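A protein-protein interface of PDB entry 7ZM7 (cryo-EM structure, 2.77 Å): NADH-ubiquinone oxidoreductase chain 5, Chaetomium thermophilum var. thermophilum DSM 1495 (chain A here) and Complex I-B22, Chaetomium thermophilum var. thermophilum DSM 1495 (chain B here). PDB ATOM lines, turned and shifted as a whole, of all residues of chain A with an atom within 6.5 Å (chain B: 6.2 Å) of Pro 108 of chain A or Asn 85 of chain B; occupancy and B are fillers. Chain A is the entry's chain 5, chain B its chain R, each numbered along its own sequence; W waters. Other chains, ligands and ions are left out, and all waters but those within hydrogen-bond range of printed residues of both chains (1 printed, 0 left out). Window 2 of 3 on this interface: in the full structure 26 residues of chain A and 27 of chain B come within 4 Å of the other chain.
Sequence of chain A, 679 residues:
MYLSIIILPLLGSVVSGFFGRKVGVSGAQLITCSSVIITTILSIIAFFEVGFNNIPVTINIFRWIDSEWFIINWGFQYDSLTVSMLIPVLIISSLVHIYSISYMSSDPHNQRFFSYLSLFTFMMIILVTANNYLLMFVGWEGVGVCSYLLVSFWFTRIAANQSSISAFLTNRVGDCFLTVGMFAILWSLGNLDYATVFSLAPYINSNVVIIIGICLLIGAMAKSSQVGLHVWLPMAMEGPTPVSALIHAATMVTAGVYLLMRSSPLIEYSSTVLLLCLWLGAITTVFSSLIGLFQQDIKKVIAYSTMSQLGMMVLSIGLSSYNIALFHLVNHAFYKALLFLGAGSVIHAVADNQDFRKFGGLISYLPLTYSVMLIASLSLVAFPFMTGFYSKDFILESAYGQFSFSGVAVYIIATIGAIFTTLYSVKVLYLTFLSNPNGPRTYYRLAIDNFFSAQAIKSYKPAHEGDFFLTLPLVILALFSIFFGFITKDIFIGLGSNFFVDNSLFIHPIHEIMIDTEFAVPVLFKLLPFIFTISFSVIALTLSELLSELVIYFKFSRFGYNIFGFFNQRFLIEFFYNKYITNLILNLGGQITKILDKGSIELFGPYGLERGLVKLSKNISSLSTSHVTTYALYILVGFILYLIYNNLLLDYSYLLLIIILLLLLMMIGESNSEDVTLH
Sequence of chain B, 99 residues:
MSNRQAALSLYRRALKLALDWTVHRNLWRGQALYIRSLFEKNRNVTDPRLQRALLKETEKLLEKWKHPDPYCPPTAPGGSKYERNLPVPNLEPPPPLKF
The side-chain carboxylate (OD1) of Asp 107 of chain A lies within hydrogen-bond range of the backbone NH (N) of His 109 of chain A, at 3.0 Å. OD1 of Asn 110 of chain A lies close to O of Asp 107 of chain A (2.8 Å). The side-chain carboxylate (OD2) of Asp 107 of chain A lies within hydrogen-bond range of the indole nitrogen (NE1) of Trp 154 of chain A (2.8 Å).
Of the 7 printed residues of chain B, 6 touch a printed residue of chain A. Hydrophobic or aromatic side chains of chain B that line the printed part of chain A: Leu 86. Hydrophobic or aromatic side chains of chain A within 4 Å of the printed part of chain B: Pro 108 and Trp 154. Along chain A the printed residues that touch a printed residue of chain B span positions 107 to 157. Among the printed residues, no Asp or Glu carboxylate lies within 4 Å of a Lys or Arg side-chain nitrogen of the other chain.
Water W1 bridges the side-chain carboxylate of Glu 83 of chain B and the backbone carbonyl oxygen of Thr 156 of chain A.
Among the printed residues, pairs that only touch across the chains: Asp 107 of chain A with Asn 85 of chain B, Pro 108 of chain A with Asn 85 of chain B, Trp 154 of chain A with Arg 84 of chain B, Trp 154 of chain A with Asn 85 of chain B, Thr 156 of chain A with Leu 86 of chain B and Arg 157 of chain A with Lys 81 of chain B.
The backbone carbonyl oxygen of Tyr 82 of chain B is in hydrogen-bond range of the guanidinium group of Arg 157 of chain A, at 3.2 Å. OG1 of Thr 156 of chain A sits close to O of Glu 83 of chain B, 3.4 Å away. O of Glu 83 of chain B sits at hydrogen-bond distance from N of Arg 157 of chain A (3.3 Å). The backbone carbonyl oxygen of Arg 84 of chain B is in hydrogen-bond range of the side-chain hydroxyl of Thr 156 of chain A (2.9 Å).
Of chain B, only Asn 85 (3.9 Å) comes within 4 Å of Pro 108 of chain A. Of the printed residues of chain A, Arg 84 of chain B touches Trp 154 and Thr 156. Printed residues of chain A within 4 Å of Lys 81 of chain B: Arg 157 (3.8 Å). The nearest printed residue of chain A that does not touch Glu 83 of chain B is Trp 154 of chain A (5.1 Å).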
ATOM      1  N   VAL A  25       6.936  21.477 -12.858  1.00  0.00           N
ATOM      2  CA  VAL A  25       7.021  20.105 -12.379  1.00  0.00           C
ATOM      3  C   VAL A  25       6.029  19.222 -13.117  1.00  0.00           C
ATOM      4  O   VAL A  25       6.353  18.112 -13.541  1.00  0.00           O
ATOM      5  CB  VAL A  25       6.795  20.068 -10.862  1.00  0.00           C
ATOM      6  CG1 VAL A  25       6.784  18.642 -10.371  1.00  0.00           C
ATOM      7  CG2 VAL A  25       7.838  20.874 -10.170  1.00  0.00           C
ATOM      8  N   MET A 104       8.015  10.400  -6.128  1.00  0.00           N
ATOM      9  CA  MET A 104       8.850  11.568  -5.903  1.00  0.00           C
ATOM     10  C   MET A 104       8.029  12.839  -5.735  1.00  0.00           C
ATOM     11  O   MET A 104       8.573  13.942  -5.833  1.00  0.00           O
ATOM     12  CB  MET A 104       9.852  11.720  -7.047  1.00  0.00           C
ATOM     13  CG  MET A 104      10.764  10.531  -7.240  1.00  0.00           C
ATOM     14  SD  MET A 104      11.758  10.159  -5.795  1.00  0.00           S
ATOM     15  CE  MET A 104      13.272  11.012  -6.168  1.00  0.00           C
ATOM     16  N   SER A 105       6.741  12.699  -5.437  1.00  0.00           N
ATOM     17  CA  SER A 105       5.828  13.837  -5.445  1.00  0.00           C
ATOM     18  C   SER A 105       6.229  14.917  -4.449  1.00  0.00           C
ATOM     19  O   SER A 105       6.026  16.105  -4.719  1.00  0.00           O
ATOM     20  CB  SER A 105       4.406  13.348  -5.185  1.00  0.00           C
ATOM     21  OG  SER A 105       4.297  12.798  -3.888  1.00  0.00           O
ATOM     22  N   SER A 106       6.820  14.544  -3.319  1.00  0.00           N
ATOM     23  CA  SER A 106       7.236  15.515  -2.318  1.00  0.00           C
ATOM     24  C   SER A 106       8.657  16.035  -2.515  1.00  0.00           C
ATOM     25  O   SER A 106       9.054  16.970  -1.818  1.00  0.00           O
ATOM     26  CB  SER A 106       7.114  14.900  -0.927  1.00  0.00           C
ATOM     27  OG  SER A 106       7.817  13.677  -0.855  1.00  0.00           O
ATOM     28  N   ASP A 107       9.423  15.465  -3.437  1.00  0.00           N
ATOM     29  CA  ASP A 107      10.811  15.855  -3.601  1.00  0.00           C
ATOM     30  C   ASP A 107      10.918  17.255  -4.197  1.00  0.00           C
ATOM     31  O   ASP A 107      10.148  17.613  -5.091  1.00  0.00           O
ATOM     32  CB  ASP A 107      11.539  14.847  -4.491  1.00  0.00           C
ATOM     33  CG  ASP A 107      13.048  14.932  -4.363  1.00  0.00           C
ATOM     34  OD1 ASP A 107      13.681  15.729  -5.081  1.00  0.00           O
ATOM     35  OD2 ASP A 107      13.600  14.233  -3.502  1.00  0.00           O
ATOM     36  N   PRO A 108      11.873  18.059  -3.738  1.00  0.00           N
ATOM     37  CA  PRO A 108      12.033  19.404  -4.307  1.00  0.00           C
ATOM     38  C   PRO A 108      12.341  19.413  -5.785  1.00  0.00           C
ATOM     39  O   PRO A 108      11.922  20.338  -6.486  1.00  0.00           O
ATOM     40  CB  PRO A 108      13.197  19.984  -3.496  1.00  0.00           C
ATOM     41  CG  PRO A 108      13.292  19.137  -2.297  1.00  0.00           C
ATOM     42  CD  PRO A 108      12.820  17.798  -2.646  1.00  0.00           C
ATOM     43  N   HIS A 109      13.046  18.408  -6.287  1.00  0.00           N
ATOM     44  CA  HIS A 109      13.643  18.427  -7.616  1.00  0.00           C
ATOM     45  C   HIS A 109      13.070  17.303  -8.466  1.00  0.00           C
ATOM     46  O   HIS A 109      13.655  16.227  -8.564  1.00  0.00           O
ATOM     47  CB  HIS A 109      15.153  18.331  -7.491  1.00  0.00           C
ATOM     48  CG  HIS A 109      15.716  19.181  -6.399  1.00  0.00           C
ATOM     49  ND1 HIS A 109      15.467  20.529  -6.309  1.00  0.00           N
ATOM     50  CD2 HIS A 109      16.508  18.877  -5.347  1.00  0.00           C
ATOM     51  CE1 HIS A 109      16.074  21.017  -5.247  1.00  0.00           C
ATOM     52  NE2 HIS A 109      16.720  20.036  -4.651  1.00  0.00           N
ATOM     53  N   ASN A 110      11.938  17.556  -9.104  1.00  0.00           N
ATOM     54  CA  ASN A 110      11.330  16.560  -9.970  1.00  0.00           C
ATOM     55  C   ASN A 110      11.747  16.702 -11.411  1.00  0.00           C
ATOM     56  O   ASN A 110      11.869  15.696 -12.109  1.00  0.00           O
ATOM     57  CB  ASN A 110       9.805  16.635  -9.896  1.00  0.00           C
ATOM     58  CG  ASN A 110       9.274  16.258  -8.545  1.00  0.00           C
ATOM     59  OD1 ASN A 110       9.125  17.099  -7.666  1.00  0.00           O
ATOM     60  ND2 ASN A 110       8.951  14.997  -8.380  1.00  0.00           N
ATOM     61  N   GLN A 111      11.953  17.931 -11.872  1.00  0.00           N
ATOM     62  CA  GLN A 111      12.372  18.135 -13.246  1.00  0.00           C
ATOM     63  C   GLN A 111      13.740  17.517 -13.498  1.00  0.00           C
ATOM     64  O   GLN A 111      14.028  17.068 -14.608  1.00  0.00           O
ATOM     65  CB  GLN A 111      12.389  19.622 -13.578  1.00  0.00           C
ATOM     66  CG  GLN A 111      11.054  20.325 -13.624  1.00  0.00           C
ATOM     67  CD  GLN A 111      10.808  21.208 -12.421  1.00  0.00           C
ATOM     68  OE1 GLN A 111      11.397  21.028 -11.362  1.00  0.00           O
ATOM     69  NE2 GLN A 111      10.003  22.231 -12.613  1.00  0.00           N
ATOM     70  N   PHE A 153      21.440  11.181  -6.686  1.00  0.00           N
ATOM     71  CA  PHE A 153      20.441  12.214  -6.916  1.00  0.00           C
ATOM     72  C   PHE A 153      20.307  13.129  -5.706  1.00  0.00           C
ATOM     73  O   PHE A 153      20.241  14.353  -5.846  1.00  0.00           O
ATOM     74  CB  PHE A 153      19.109  11.573  -7.271  1.00  0.00           C
ATOM     75  CG  PHE A 153      18.024  12.562  -7.518  1.00  0.00           C
ATOM     76  CD1 PHE A 153      18.096  13.435  -8.585  1.00  0.00           C
ATOM     77  CD2 PHE A 153      16.943  12.643  -6.666  1.00  0.00           C
ATOM     78  CE1 PHE A 153      17.122  14.339  -8.787  1.00  0.00           C
ATOM     79  CE2 PHE A 153      15.979  13.547  -6.883  1.00  0.00           C
ATOM     80  CZ  PHE A 153      16.067  14.397  -7.939  1.00  0.00           C
ATOM     81  N   TRP A 154      20.283  12.556  -4.509  1.00  0.00           N
ATOM     82  CA  TRP A 154      20.370  13.343  -3.284  1.00  0.00           C
ATOM     83  C   TRP A 154      21.845  13.532  -2.969  1.00  0.00           C
ATOM     84  O   TRP A 154      22.429  12.855  -2.127  1.00  0.00           O
ATOM     85  CB  TRP A 154      19.625  12.660  -2.149  1.00  0.00           C
ATOM     86  CG  TRP A 154      18.161  12.487  -2.391  1.00  0.00           C
ATOM     87  CD1 TRP A 154      17.258  13.467  -2.660  1.00  0.00           C
ATOM     88  CD2 TRP A 154      17.428  11.262  -2.378  1.00  0.00           C
ATOM     89  NE1 TRP A 154      16.009  12.932  -2.812  1.00  0.00           N
ATOM     90  CE2 TRP A 154      16.085  11.578  -2.642  1.00  0.00           C
ATOM     91  CE3 TRP A 154      17.774   9.933  -2.155  1.00  0.00           C
ATOM     92  CZ2 TRP A 154      15.097  10.613  -2.700  1.00  0.00           C
ATOM     93  CZ3 TRP A 154      16.794   8.987  -2.199  1.00  0.00           C
ATOM     94  CH2 TRP A 154      15.471   9.328  -2.471  1.00  0.00           C
ATOM     95  N   THR A 156      23.428  15.545  -1.322  1.00  0.00           N
ATOM     96  CA  THR A 156      23.810  16.039  -0.010  1.00  0.00           C
ATOM     97  C   THR A 156      24.037  14.925   0.999  1.00  0.00           C
ATOM     98  O   THR A 156      24.411  15.209   2.136  1.00  0.00           O
ATOM     99  CB  THR A 156      22.763  17.024   0.518  1.00  0.00           C
ATOM    100  OG1 THR A 156      21.456  16.474   0.354  1.00  0.00           O
ATOM    101  CG2 THR A 156      22.852  18.320  -0.247  1.00  0.00           C
ATOM    102  N   ARG A 157      23.831  13.677   0.613  1.00  0.00           N
ATOM    103  CA  ARG A 157      24.084  12.532   1.473  1.00  0.00           C
ATOM    104  C   ARG A 157      25.444  11.941   1.121  1.00  0.00           C
ATOM    105  O   ARG A 157      25.649  11.487  -0.008  1.00  0.00           O
ATOM    106  CB  ARG A 157      22.977  11.497   1.307  1.00  0.00           C
ATOM    107  CG  ARG A 157      23.116  10.280   2.181  1.00  0.00           C
ATOM    108  CD  ARG A 157      21.934   9.375   2.001  1.00  0.00           C
ATOM    109  NE  ARG A 157      22.279   7.985   2.259  1.00  0.00           N
ATOM    110  CZ  ARG A 157      22.061   7.358   3.405  1.00  0.00           C
ATOM    111  NH1 ARG A 157      21.497   7.990   4.412  1.00  0.00           N
ATOM    112  NH2 ARG A 157      22.405   6.100   3.542  1.00  0.00           N
ATOM    113  N   LYS B  81      17.856   7.614   5.428  1.00  0.00           N
ATOM    114  CA  LYS B  81      17.286   8.886   4.899  1.00  0.00           C
ATOM    115  C   LYS B  81      18.070  10.055   5.490  1.00  0.00           C
ATOM    116  O   LYS B  81      17.671  11.210   5.284  1.00  0.00           O
ATOM    117  CB  LYS B  81      15.797   8.975   5.246  1.00  0.00           C
ATOM    118  CG  LYS B  81      14.974   9.910   4.375  1.00  0.00           C
ATOM    119  CD  LYS B  81      13.576  10.144   4.885  1.00  0.00           C
ATOM    120  CE  LYS B  81      12.871  11.238   4.115  1.00  0.00           C
ATOM    121  NZ  LYS B  81      13.706  12.459   4.028  1.00  0.00           N
ATOM    122  N   TYR B  82      19.153   9.750   6.200  1.00  0.00           N
ATOM    123  CA  TYR B  82      19.963  10.806   6.854  1.00  0.00           C
ATOM    124  C   TYR B  82      20.582  11.718   5.791  1.00  0.00           C
ATOM    125  O   TYR B  82      21.068  11.189   4.786  1.00  0.00           O
ATOM    126  CB  TYR B  82      21.027  10.167   7.740  1.00  0.00           C
ATOM    127  CG  TYR B  82      21.823  11.140   8.570  1.00  0.00           C
ATOM    128  CD1 TYR B  82      21.195  12.111   9.329  1.00  0.00           C
ATOM    129  CD2 TYR B  82      23.204  11.076   8.612  1.00  0.00           C
ATOM    130  CE1 TYR B  82      21.918  13.002  10.102  1.00  0.00           C
ATOM    131  CE2 TYR B  82      23.943  11.956   9.383  1.00  0.00           C
ATOM    132  CZ  TYR B  82      23.298  12.923  10.129  1.00  0.00           C
ATOM    133  OH  TYR B  82      24.021  13.798  10.888  1.00  0.00           O
ATOM    134  N   GLU B  83      20.543  13.033   6.012  1.00  0.00           N
ATOM    135  CA  GLU B  83      21.169  14.017   5.089  1.00  0.00           C
ATOM    136  C   GLU B  83      20.610  13.876   3.677  1.00  0.00           C
ATOM    137  O   GLU B  83      21.371  14.094   2.738  1.00  0.00           O
ATOM    138  CB  GLU B  83      22.685  13.837   5.097  1.00  0.00           C
ATOM    139  CG  GLU B  83      23.329  14.173   6.425  1.00  0.00           C
ATOM    140  CD  GLU B  83      24.820  13.900   6.454  1.00  0.00           C
ATOM    141  OE1 GLU B  83      25.303  13.196   5.547  1.00  0.00           O
ATOM    142  OE2 GLU B  83      25.495  14.399   7.374  1.00  0.00           O
ATOM    143  N   ARG B  84      19.320  13.577   3.527  1.00  0.00           N
ATOM    144  CA  ARG B  84      18.782  13.293   2.174  1.00  0.00           C
ATOM    145  C   ARG B  84      18.572  14.605   1.435  1.00  0.00           C
ATOM    146  O   ARG B  84      19.111  14.759   0.320  1.00  0.00           O
ATOM    147  CB  ARG B  84      17.489  12.479   2.228  1.00  0.00           C
ATOM    148  CG  ARG B  84      16.705  12.474   0.926  1.00  0.00           C
ATOM    149  CD  ARG B  84      15.570  11.475   0.910  1.00  0.00           C
ATOM    150  NE  ARG B  84      16.062  10.113   1.041  1.00  0.00           N
ATOM    151  CZ  ARG B  84      15.291   9.036   1.010  1.00  0.00           C
ATOM    152  NH1 ARG B  84      13.988   9.164   0.841  1.00  0.00           N
ATOM    153  NH2 ARG B  84      15.823   7.837   1.144  1.00  0.00           N
ATOM    154  N   ASN B  85      17.838  15.525   2.041  1.00  0.00           N
ATOM    155  CA  ASN B  85      17.557  16.770   1.359  1.00  0.00           C
ATOM    156  C   ASN B  85      17.983  17.936   2.230  1.00  0.00           C
ATOM    157  O   ASN B  85      17.187  18.839   2.500  1.00  0.00           O
ATOM    158  CB  ASN B  85      16.083  16.849   0.999  1.00  0.00           C
ATOM    159  CG  ASN B  85      15.802  16.293  -0.368  1.00  0.00           C
ATOM    160  OD1 ASN B  85      16.372  16.739  -1.364  1.00  0.00           O
ATOM    161  ND2 ASN B  85      14.935  15.303  -0.428  1.00  0.00           N
ATOM    162  N   LEU B  86      19.222  17.894   2.703  1.00  0.00           N
ATOM    163  CA  LEU B  86      19.728  18.902   3.616  1.00  0.00           C
ATOM    164  C   LEU B  86      19.539  20.286   3.020  1.00  0.00           C
ATOM    165  O   LEU B  86      19.970  20.525   1.884  1.00  0.00           O
ATOM    166  CB  LEU B  86      21.211  18.697   3.886  1.00  0.00           C
ATOM    167  CG  LEU B  86      21.676  17.805   5.016  1.00  0.00           C
ATOM    168  CD1 LEU B  86      23.134  17.573   4.836  1.00  0.00           C
ATOM    169  CD2 LEU B  86      21.410  18.468   6.335  1.00  0.00           C
ATOM    170  N   PRO B  87      18.928  21.220   3.747  1.00  0.00           N
ATOM    171  CA  PRO B  87      18.780  22.581   3.228  1.00  0.00           C
ATOM    172  C   PRO B  87      20.120  23.277   3.128  1.00  0.00           C
ATOM    173  O   PRO B  87      21.110  22.866   3.730  1.00  0.00           O
ATOM    174  CB  PRO B  87      17.881  23.260   4.262  1.00  0.00           C
ATOM    175  CG  PRO B  87      18.072  22.465   5.501  1.00  0.00           C
ATOM    176  CD  PRO B  87      18.278  21.059   5.056  1.00  0.00           C
HETATM  177  O   HOH W   1      26.728  15.727   4.471  1.00  0.00           O
